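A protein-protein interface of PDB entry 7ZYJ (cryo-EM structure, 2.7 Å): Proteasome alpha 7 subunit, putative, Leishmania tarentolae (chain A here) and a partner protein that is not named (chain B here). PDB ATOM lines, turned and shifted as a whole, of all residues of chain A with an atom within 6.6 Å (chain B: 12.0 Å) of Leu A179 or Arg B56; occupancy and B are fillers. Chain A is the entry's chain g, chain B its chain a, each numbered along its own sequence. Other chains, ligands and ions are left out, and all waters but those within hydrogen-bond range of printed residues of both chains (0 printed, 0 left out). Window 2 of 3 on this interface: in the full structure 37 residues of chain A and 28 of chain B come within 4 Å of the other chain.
NH1 of Arg B56 is in salt-bridge range of OE1 of Glu A177 (2.8 Å). The backbone carbonyl oxygen (O) of Leu B57 lies within hydrogen-bond range of the backbone NH (N) of Tyr A161 (2.8 Å).
O of Pro B60 is in hydrogen-bond range of NE2 of His B51 (2.7 Å). O of Arg B59 lies within hydrogen-bond range of OG of Ser B62 (2.7 Å). NE of Arg B59 lies within salt-bridge range of OD1 of Asp B61 (3.7 Å). OD1 of Asp B55 lies within hydrogen-bond range of N of Leu B57 (3.1 Å).
Tyr A161 touches Met B58. OH of Tyr A161 touches CG of Arg B59, 3.6 Å away. Tyr A161 touches Pro B60. CB of Leu A176 touches CD1 of Leu B57, at 3.8 Å. OE2 of Glu A177 touches CG of Leu B57, 3.7 Å away. Leu A179 touches Arg B56 (O to NH2, 3.5 Å). CE2 of Phe A181 touches CD2 of Leu B57, 3.5 Å away.
Of the printed residues of chain A, Arg B56 touches Glu A177 (2.8 Å) and Leu A179 (3.5 Å). Of chain B, only Leu B57 (2.8 Å), Met B58 (3.9 Å), Arg B59 (3.6 Å) and Pro B60 (3.5 Å) come within 4 Å of Tyr A161. Of chain B, only Arg B56 (2.8 Å) and Leu B57 (3.7 Å) come within 4 Å of Glu A177. No residue of chain B comes within 4 Å of Lys A178. No residue of chain B comes within 4 Å of Asp A180. Phe A181 touches just one residue of chain B: Leu B57. No residue of chain B comes within 4 Å of Ala A189. No residue of chain B comes within 4 Å of Lys A192. Printed residues of chain A within 4 Å of Leu B57: Tyr A161 (2.8 Å), Leu A176 (3.8 Å), Glu A177 (3.7 Å) and Phe A181 (3.5 Å). Printed residues of chain A within 4 Å of Pro B60: Tyr A161 (3.5 Å). Printed residues of chain A within 4 Å of Arg B59: Tyr A161. Val B63 touches none of the printed residues of chain A.
Of the 14 printed residues of chain B, 5 touch a printed residue of chain A. Hydrophobic or aromatic side chains of chain B that line the printed part of chain A: Leu B57 and Pro B60. Hydrophobic or aromatic side chains of chain A that line the printed part of chain B: Tyr A161, Leu A176 and Phe A181. Along chain A the printed residues that touch a printed residue of chain B span positions 161 to 181. Among the printed residues, 9 pairs touch across the chains. Among the printed residues, Asp or Glu carboxylates within 4 Å of a Lys or Arg side-chain nitrogen of the other chain: Glu A177 with Arg B56.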
ATOM      1  N   ALA A  40       4.899   3.271   7.578  1.00  0.00           N
ATOM      2  CA  ALA A  40       5.449   4.620   7.568  1.00  0.00           C
ATOM      3  C   ALA A  40       6.150   4.906   8.887  1.00  0.00           C
ATOM      4  O   ALA A  40       5.622   4.585   9.957  1.00  0.00           O
ATOM      5  CB  ALA A  40       4.351   5.659   7.322  1.00  0.00           C
ATOM      6  N   TYR A 161      11.520   4.979   5.224  1.00  0.00           N
ATOM      7  CA  TYR A 161      10.585   5.955   5.767  1.00  0.00           C
ATOM      8  C   TYR A 161       9.148   5.540   5.486  1.00  0.00           C
ATOM      9  O   TYR A 161       8.284   5.651   6.361  1.00  0.00           O
ATOM     10  CB  TYR A 161      10.851   7.340   5.173  1.00  0.00           C
ATOM     11  CG  TYR A 161      12.255   7.852   5.390  1.00  0.00           C
ATOM     12  CD1 TYR A 161      12.712   8.162   6.662  1.00  0.00           C
ATOM     13  CD2 TYR A 161      13.121   8.030   4.320  1.00  0.00           C
ATOM     14  CE1 TYR A 161      13.995   8.632   6.864  1.00  0.00           C
ATOM     15  CE2 TYR A 161      14.404   8.497   4.512  1.00  0.00           C
ATOM     16  CZ  TYR A 161      14.837   8.797   5.785  1.00  0.00           C
ATOM     17  OH  TYR A 161      16.116   9.265   5.980  1.00  0.00           O
ATOM     18  N   SER A 174       3.329   4.635  -4.951  1.00  0.00           N
ATOM     19  CA  SER A 174       3.113   5.950  -5.544  1.00  0.00           C
ATOM     20  C   SER A 174       2.301   6.851  -4.623  1.00  0.00           C
ATOM     21  O   SER A 174       2.606   8.043  -4.495  1.00  0.00           O
ATOM     22  CB  SER A 174       2.416   5.808  -6.897  1.00  0.00           C
ATOM     23  OG  SER A 174       1.099   5.311  -6.741  1.00  0.00           O
ATOM     24  N   GLU A 175       1.266   6.306  -3.980  1.00  0.00           N
ATOM     25  CA  GLU A 175       0.521   7.083  -2.993  1.00  0.00           C
ATOM     26  C   GLU A 175       1.397   7.473  -1.809  1.00  0.00           C
ATOM     27  O   GLU A 175       1.261   8.580  -1.277  1.00  0.00           O
ATOM     28  CB  GLU A 175      -0.702   6.305  -2.506  1.00  0.00           C
ATOM     29  CG  GLU A 175      -1.624   5.823  -3.613  1.00  0.00           C
ATOM     30  CD  GLU A 175      -2.569   6.905  -4.096  1.00  0.00           C
ATOM     31  OE1 GLU A 175      -2.931   7.784  -3.285  1.00  0.00           O
ATOM     32  OE2 GLU A 175      -2.949   6.876  -5.284  1.00  0.00           O
ATOM     33  N   LEU A 176       2.292   6.579  -1.382  1.00  0.00           N
ATOM     34  CA  LEU A 176       3.193   6.898  -0.279  1.00  0.00           C
ATOM     35  C   LEU A 176       4.192   7.982  -0.659  1.00  0.00           C
ATOM     36  O   LEU A 176       4.646   8.734   0.210  1.00  0.00           O
ATOM     37  CB  LEU A 176       3.928   5.639   0.180  1.00  0.00           C
ATOM     38  CG  LEU A 176       3.145   4.689   1.087  1.00  0.00           C
ATOM     39  CD1 LEU A 176       3.917   3.399   1.308  1.00  0.00           C
ATOM     40  CD2 LEU A 176       2.830   5.360   2.412  1.00  0.00           C
ATOM     41  N   GLU A 177       4.548   8.079  -1.942  1.00  0.00           N
ATOM     42  CA  GLU A 177       5.469   9.123  -2.383  1.00  0.00           C
ATOM     43  C   GLU A 177       4.882  10.520  -2.235  1.00  0.00           C
ATOM     44  O   GLU A 177       5.631  11.501  -2.294  1.00  0.00           O
ATOM     45  CB  GLU A 177       5.880   8.892  -3.838  1.00  0.00           C
ATOM     46  CG  GLU A 177       6.684   7.625  -4.073  1.00  0.00           C
ATOM     47  CD  GLU A 177       8.167   7.821  -3.830  1.00  0.00           C
ATOM     48  OE1 GLU A 177       8.562   8.926  -3.404  1.00  0.00           O
ATOM     49  OE2 GLU A 177       8.939   6.868  -4.065  1.00  0.00           O
ATOM     50  N   LYS A 178       3.568  10.635  -2.048  1.00  0.00           N
ATOM     51  CA  LYS A 178       2.919  11.930  -1.900  1.00  0.00           C
ATOM     52  C   LYS A 178       2.945  12.454  -0.470  1.00  0.00           C
ATOM     53  O   LYS A 178       2.500  13.582  -0.233  1.00  0.00           O
ATOM     54  CB  LYS A 178       1.469  11.851  -2.386  1.00  0.00           C
ATOM     55  CG  LYS A 178       1.329  11.611  -3.879  1.00  0.00           C
ATOM     56  CD  LYS A 178      -0.122  11.691  -4.317  1.00  0.00           C
ATOM     57  CE  LYS A 178      -0.900  10.464  -3.874  1.00  0.00           C
ATOM     58  NZ  LYS A 178      -2.298  10.477  -4.389  1.00  0.00           N
ATOM     59  N   LEU A 179       3.447  11.674   0.481  1.00  0.00           N
ATOM     60  CA  LEU A 179       3.547  12.119   1.860  1.00  0.00           C
ATOM     61  C   LEU A 179       4.897  12.794   2.106  1.00  0.00           C
ATOM     62  O   LEU A 179       5.839  12.668   1.321  1.00  0.00           O
ATOM     63  CB  LEU A 179       3.346  10.945   2.820  1.00  0.00           C
ATOM     64  CG  LEU A 179       2.087  10.096   2.633  1.00  0.00           C
ATOM     65  CD1 LEU A 179       1.856   9.213   3.847  1.00  0.00           C
ATOM     66  CD2 LEU A 179       0.869  10.971   2.373  1.00  0.00           C
ATOM     67  N   ASP A 180       4.980  13.520   3.219  1.00  0.00           N
ATOM     68  CA  ASP A 180       6.171  14.294   3.541  1.00  0.00           C
ATOM     69  C   ASP A 180       7.141  13.521   4.431  1.00  0.00           C
ATOM     70  O   ASP A 180       8.359  13.610   4.243  1.00  0.00           O
ATOM     71  CB  ASP A 180       5.767  15.613   4.208  1.00  0.00           C
ATOM     72  CG  ASP A 180       6.961  16.443   4.630  1.00  0.00           C
ATOM     73  OD1 ASP A 180       7.618  17.037   3.749  1.00  0.00           O
ATOM     74  OD2 ASP A 180       7.237  16.508   5.844  1.00  0.00           O
ATOM     75  N   PHE A 181       6.614  12.793   5.419  1.00  0.00           N
ATOM     76  CA  PHE A 181       7.390  11.923   6.302  1.00  0.00           C
ATOM     77  C   PHE A 181       8.313  12.699   7.235  1.00  0.00           C
ATOM     78  O   PHE A 181       8.998  12.102   8.071  1.00  0.00           O
ATOM     79  CB  PHE A 181       8.195  10.903   5.490  1.00  0.00           C
ATOM     80  CG  PHE A 181       7.347   9.861   4.822  1.00  0.00           C
ATOM     81  CD1 PHE A 181       6.608   8.965   5.576  1.00  0.00           C
ATOM     82  CD2 PHE A 181       7.284   9.780   3.442  1.00  0.00           C
ATOM     83  CE1 PHE A 181       5.827   8.006   4.967  1.00  0.00           C
ATOM     84  CE2 PHE A 181       6.501   8.823   2.828  1.00  0.00           C
ATOM     85  CZ  PHE A 181       5.773   7.934   3.591  1.00  0.00           C
ATOM     86  N   SER A 182       8.342  14.025   7.107  1.00  0.00           N
ATOM     87  CA  SER A 182       9.039  14.870   8.068  1.00  0.00           C
ATOM     88  C   SER A 182       8.086  15.620   8.984  1.00  0.00           C
ATOM     89  O   SER A 182       8.347  15.719  10.187  1.00  0.00           O
ATOM     90  CB  SER A 182       9.943  15.874   7.344  1.00  0.00           C
ATOM     91  OG  SER A 182      10.969  15.210   6.627  1.00  0.00           O
ATOM     92  N   LEU A 184       4.907  14.490   8.991  1.00  0.00           N
ATOM     93  CA  LEU A 184       3.873  13.485   9.187  1.00  0.00           C
ATOM     94  C   LEU A 184       3.911  12.950  10.613  1.00  0.00           C
ATOM     95  O   LEU A 184       4.980  12.642  11.147  1.00  0.00           O
ATOM     96  CB  LEU A 184       4.055  12.342   8.188  1.00  0.00           C
ATOM     97  CG  LEU A 184       3.039  11.201   8.245  1.00  0.00           C
ATOM     98  CD1 LEU A 184       1.627  11.727   8.042  1.00  0.00           C
ATOM     99  CD2 LEU A 184       3.370  10.138   7.212  1.00  0.00           C
ATOM    100  N   ALA A 189      -1.032   9.623  10.136  1.00  0.00           N
ATOM    101  CA  ALA A 189      -0.467   8.549   9.328  1.00  0.00           C
ATOM    102  C   ALA A 189      -1.350   7.310   9.342  1.00  0.00           C
ATOM    103  O   ALA A 189      -1.422   6.596   8.336  1.00  0.00           O
ATOM    104  CB  ALA A 189       0.938   8.198   9.811  1.00  0.00           C
ATOM    105  N   LYS A 192      -3.973   8.055   6.842  1.00  0.00           N
ATOM    106  CA  LYS A 192      -3.382   8.072   5.508  1.00  0.00           C
ATOM    107  C   LYS A 192      -3.160   6.657   4.986  1.00  0.00           C
ATOM    108  O   LYS A 192      -3.513   6.343   3.844  1.00  0.00           O
ATOM    109  CB  LYS A 192      -2.065   8.849   5.529  1.00  0.00           C
ATOM    110  CG  LYS A 192      -2.226  10.357   5.599  1.00  0.00           C
ATOM    111  CD  LYS A 192      -2.905  10.898   4.354  1.00  0.00           C
ATOM    112  CE  LYS A 192      -3.171  12.390   4.477  1.00  0.00           C
ATOM    113  NZ  LYS A 192      -3.827  12.938   3.258  1.00  0.00           N
ATOM    114  N   LEU A 193      -2.578   5.788   5.815  1.00  0.00           N
ATOM    115  CA  LEU A 193      -2.321   4.416   5.390  1.00  0.00           C
ATOM    116  C   LEU A 193      -3.619   3.655   5.158  1.00  0.00           C
ATOM    117  O   LEU A 193      -3.732   2.893   4.189  1.00  0.00           O
ATOM    118  CB  LEU A 193      -1.453   3.698   6.422  1.00  0.00           C
ATOM    119  CG  LEU A 193      -0.040   4.244   6.634  1.00  0.00           C
ATOM    120  CD1 LEU A 193       0.826   3.218   7.342  1.00  0.00           C
ATOM    121  CD2 LEU A 193       0.589   4.658   5.314  1.00  0.00           C
ATOM    122  N   ILE A 196      -5.039   4.847   1.869  1.00  0.00           N
ATOM    123  CA  ILE A 196      -4.280   4.300   0.747  1.00  0.00           C
ATOM    124  C   ILE A 196      -4.663   2.847   0.506  1.00  0.00           C
ATOM    125  O   ILE A 196      -4.895   2.433  -0.636  1.00  0.00           O
ATOM    126  CB  ILE A 196      -2.768   4.454   0.995  1.00  0.00           C
ATOM    127  CG1 ILE A 196      -2.361   5.927   0.929  1.00  0.00           C
ATOM    128  CG2 ILE A 196      -1.973   3.636  -0.010  1.00  0.00           C
ATOM    129  CD1 ILE A 196      -0.932   6.182   1.353  1.00  0.00           C
ATOM    130  N   HIS B  51      27.145   3.472  -3.021  1.00  0.00           N
ATOM    131  CA  HIS B  51      26.006   3.496  -2.102  1.00  0.00           C
ATOM    132  C   HIS B  51      24.911   4.328  -2.766  1.00  0.00           C
ATOM    133  O   HIS B  51      24.781   5.527  -2.517  1.00  0.00           O
ATOM    134  CB  HIS B  51      26.414   4.058  -0.737  1.00  0.00           C
ATOM    135  CG  HIS B  51      25.261   4.319   0.182  1.00  0.00           C
ATOM    136  ND1 HIS B  51      24.524   5.484   0.141  1.00  0.00           N
ATOM    137  CD2 HIS B  51      24.721   3.568   1.171  1.00  0.00           C
ATOM    138  CE1 HIS B  51      23.578   5.436   1.062  1.00  0.00           C
ATOM    139  NE2 HIS B  51      23.676   4.285   1.701  1.00  0.00           N
ATOM    140  N   LEU B  52      24.114   3.678  -3.609  1.00  0.00           N
ATOM    141  CA  LEU B  52      23.083   4.347  -4.389  1.00  0.00           C
ATOM    142  C   LEU B  52      21.716   3.850  -3.946  1.00  0.00           C
ATOM    143  O   LEU B  52      21.513   2.644  -3.771  1.00  0.00           O
ATOM    144  CB  LEU B  52      23.312   4.131  -5.893  1.00  0.00           C
ATOM    145  CG  LEU B  52      23.304   2.740  -6.538  1.00  0.00           C
ATOM    146  CD1 LEU B  52      21.899   2.247  -6.868  1.00  0.00           C
ATOM    147  CD2 LEU B  52      24.183   2.732  -7.780  1.00  0.00           C
ATOM    148  N   ILE B  53      20.791   4.784  -3.746  1.00  0.00           N
ATOM    149  CA  ILE B  53      19.463   4.484  -3.219  1.00  0.00           C
ATOM    150  C   ILE B  53      18.419   5.005  -4.199  1.00  0.00           C
ATOM    151  O   ILE B  53      17.920   6.127  -4.031  1.00  0.00           O
ATOM    152  CB  ILE B  53      19.261   5.097  -1.824  1.00  0.00           C
ATOM    153  CG1 ILE B  53      20.509   4.911  -0.958  1.00  0.00           C
ATOM    154  CG2 ILE B  53      18.049   4.486  -1.145  1.00  0.00           C
ATOM    155  CD1 ILE B  53      20.826   3.467  -0.640  1.00  0.00           C
ATOM    156  N   PRO B  54      18.077   4.242  -5.240  1.00  0.00           N
ATOM    157  CA  PRO B  54      17.053   4.724  -6.186  1.00  0.00           C
ATOM    158  C   PRO B  54      15.706   4.973  -5.529  1.00  0.00           C
ATOM    159  O   PRO B  54      14.983   5.896  -5.927  1.00  0.00           O
ATOM    160  CB  PRO B  54      16.990   3.600  -7.230  1.00  0.00           C
ATOM    161  CG  PRO B  54      17.536   2.395  -6.533  1.00  0.00           C
ATOM    162  CD  PRO B  54      18.581   2.906  -5.595  1.00  0.00           C
ATOM    163  N   ASP B  55      15.348   4.173  -4.529  1.00  0.00           N
ATOM    164  CA  ASP B  55      14.079   4.350  -3.837  1.00  0.00           C
ATOM    165  C   ASP B  55      14.160   5.567  -2.924  1.00  0.00           C
ATOM    166  O   ASP B  55      14.909   5.567  -1.942  1.00  0.00           O
ATOM    167  CB  ASP B  55      13.736   3.095  -3.039  1.00  0.00           C
ATOM    168  CG  ASP B  55      12.320   3.117  -2.490  1.00  0.00           C
ATOM    169  OD1 ASP B  55      11.590   4.098  -2.743  1.00  0.00           O
ATOM    170  OD2 ASP B  55      11.936   2.147  -1.804  1.00  0.00           O
ATOM    171  N   ARG B  56      13.388   6.601  -3.248  1.00  0.00           N
ATOM    172  CA  ARG B  56      13.350   7.819  -2.450  1.00  0.00           C
ATOM    173  C   ARG B  56      12.806   7.588  -1.047  1.00  0.00           C
ATOM    174  O   ARG B  56      13.118   8.369  -0.141  1.00  0.00           O
ATOM    175  CB  ARG B  56      12.509   8.882  -3.166  1.00  0.00           C
ATOM    176  CG  ARG B  56      12.653  10.285  -2.603  1.00  0.00           C
ATOM    177  CD  ARG B  56      11.380  11.089  -2.806  1.00  0.00           C
ATOM    178  NE  ARG B  56      10.575  11.152  -1.591  1.00  0.00           N
ATOM    179  CZ  ARG B  56       9.279  11.430  -1.565  1.00  0.00           C
ATOM    180  NH1 ARG B  56       8.603  11.674  -2.675  1.00  0.00           N
ATOM    181  NH2 ARG B  56       8.646  11.462  -0.397  1.00  0.00           N
ATOM    182  N   LEU B  57      12.015   6.537  -0.842  1.00  0.00           N
ATOM    183  CA  LEU B  57      11.426   6.248   0.457  1.00  0.00           C
ATOM    184  C   LEU B  57      12.309   5.369   1.333  1.00  0.00           C
ATOM    185  O   LEU B  57      11.910   5.043   2.456  1.00  0.00           O
ATOM    186  CB  LEU B  57      10.063   5.575   0.275  1.00  0.00           C
ATOM    187  CG  LEU B  57       8.957   6.431  -0.341  1.00  0.00           C
ATOM    188  CD1 LEU B  57       7.643   5.669  -0.373  1.00  0.00           C
ATOM    189  CD2 LEU B  57       8.807   7.740   0.413  1.00  0.00           C
ATOM    190  N   MET B  58      13.487   4.980   0.855  1.00  0.00           N
ATOM    191  CA  MET B  58      14.386   4.119   1.611  1.00  0.00           C
ATOM    192  C   MET B  58      15.337   4.970   2.443  1.00  0.00           C
ATOM    193  O   MET B  58      15.928   5.929   1.938  1.00  0.00           O
ATOM    194  CB  MET B  58      15.176   3.208   0.671  1.00  0.00           C
ATOM    195  CG  MET B  58      16.230   2.361   1.364  1.00  0.00           C
ATOM    196  SD  MET B  58      17.041   1.196   0.254  1.00  0.00           S
ATOM    197  CE  MET B  58      15.651   0.206  -0.283  1.00  0.00           C
ATOM    198  N   ARG B  59      15.475   4.618   3.713  1.00  0.00           N
ATOM    199  CA  ARG B  59      16.372   5.324   4.618  1.00  0.00           C
ATOM    200  C   ARG B  59      17.815   5.094   4.190  1.00  0.00           C
ATOM    201  O   ARG B  59      18.316   3.970   4.327  1.00  0.00           O
ATOM    202  CB  ARG B  59      16.147   4.845   6.049  1.00  0.00           C
ATOM    203  CG  ARG B  59      16.557   5.838   7.115  1.00  0.00           C
ATOM    204  CD  ARG B  59      15.776   5.609   8.395  1.00  0.00           C
ATOM    205  NE  ARG B  59      16.469   6.133   9.565  1.00  0.00           N
ATOM    206  CZ  ARG B  59      15.882   6.405  10.722  1.00  0.00           C
ATOM    207  NH1 ARG B  59      14.585   6.215  10.900  1.00  0.00           N
ATOM    208  NH2 ARG B  59      16.615   6.879  11.726  1.00  0.00           N
ATOM    209  N   PRO B  60      18.519   6.108   3.673  1.00  0.00           N
ATOM    210  CA  PRO B  60      19.827   5.868   3.046  1.00  0.00           C
ATOM    211  C   PRO B  60      20.901   5.345   3.989  1.00  0.00           C
ATOM    212  O   PRO B  60      21.799   4.617   3.556  1.00  0.00           O
ATOM    213  CB  PRO B  60      20.201   7.248   2.492  1.00  0.00           C
ATOM    214  CG  PRO B  60      19.486   8.209   3.374  1.00  0.00           C
ATOM    215  CD  PRO B  60      18.193   7.542   3.750  1.00  0.00           C
ATOM    216  N   ASP B  61      20.828   5.698   5.271  1.00  0.00           N
ATOM    217  CA  ASP B  61      21.850   5.299   6.227  1.00  0.00           C
ATOM    218  C   ASP B  61      21.590   3.937   6.853  1.00  0.00           C
ATOM    219  O   ASP B  61      22.392   3.490   7.680  1.00  0.00           O
ATOM    220  CB  ASP B  61      21.991   6.354   7.334  1.00  0.00           C
ATOM    221  CG  ASP B  61      20.701   6.585   8.094  1.00  0.00           C
ATOM    222  OD1 ASP B  61      19.663   6.016   7.699  1.00  0.00           O
ATOM    223  OD2 ASP B  61      20.726   7.336   9.090  1.00  0.00           O
ATOM    224  N   SER B  62      20.499   3.265   6.485  1.00  0.00           N
ATOM    225  CA  SER B  62      20.219   1.944   7.033  1.00  0.00           C
ATOM    226  C   SER B  62      20.984   0.859   6.284  1.00  0.00           C
ATOM    227  O   SER B  62      21.594  -0.019   6.902  1.00  0.00           O
ATOM    228  CB  SER B  62      18.716   1.667   6.988  1.00  0.00           C
ATOM    229  OG  SER B  62      18.255   1.600   5.651  1.00  0.00           O
ATOM    230  N   VAL B  63      20.964   0.906   4.957  1.00  0.00           N
ATOM    231  CA  VAL B  63      21.661  -0.086   4.148  1.00  0.00           C
ATOM    232  C   VAL B  63      23.091   0.379   3.900  1.00  0.00           C
ATOM    233  O   VAL B  63      23.331   1.531   3.521  1.00  0.00           O
ATOM    234  CB  VAL B  63      20.910  -0.348   2.832  1.00  0.00           C
ATOM    235  CG1 VAL B  63      19.538  -0.925   3.122  1.00  0.00           C
ATOM    236  CG2 VAL B  63      20.769   0.929   2.019  1.00  0.00           C
ATOM    237  N   LYS B 217      26.805  11.459  -1.799  1.00  0.00           N
ATOM    238  CA  LYS B 217      25.754  10.592  -1.284  1.00  0.00           C
ATOM    239  C   LYS B 217      25.691   9.252  -2.000  1.00  0.00           C
ATOM    240  O   LYS B 217      25.055   8.325  -1.486  1.00  0.00           O
ATOM    241  CB  LYS B 217      24.394  11.287  -1.385  1.00  0.00           C
ATOM    242  CG  LYS B 217      24.329  12.641  -0.699  1.00  0.00           C
ATOM    243  CD  LYS B 217      22.935  13.249  -0.784  1.00  0.00           C
ATOM    244  CE  LYS B 217      22.287  13.011  -2.142  1.00  0.00           C
ATOM    245  NZ  LYS B 217      23.084  13.586  -3.263  1.00  0.00           N
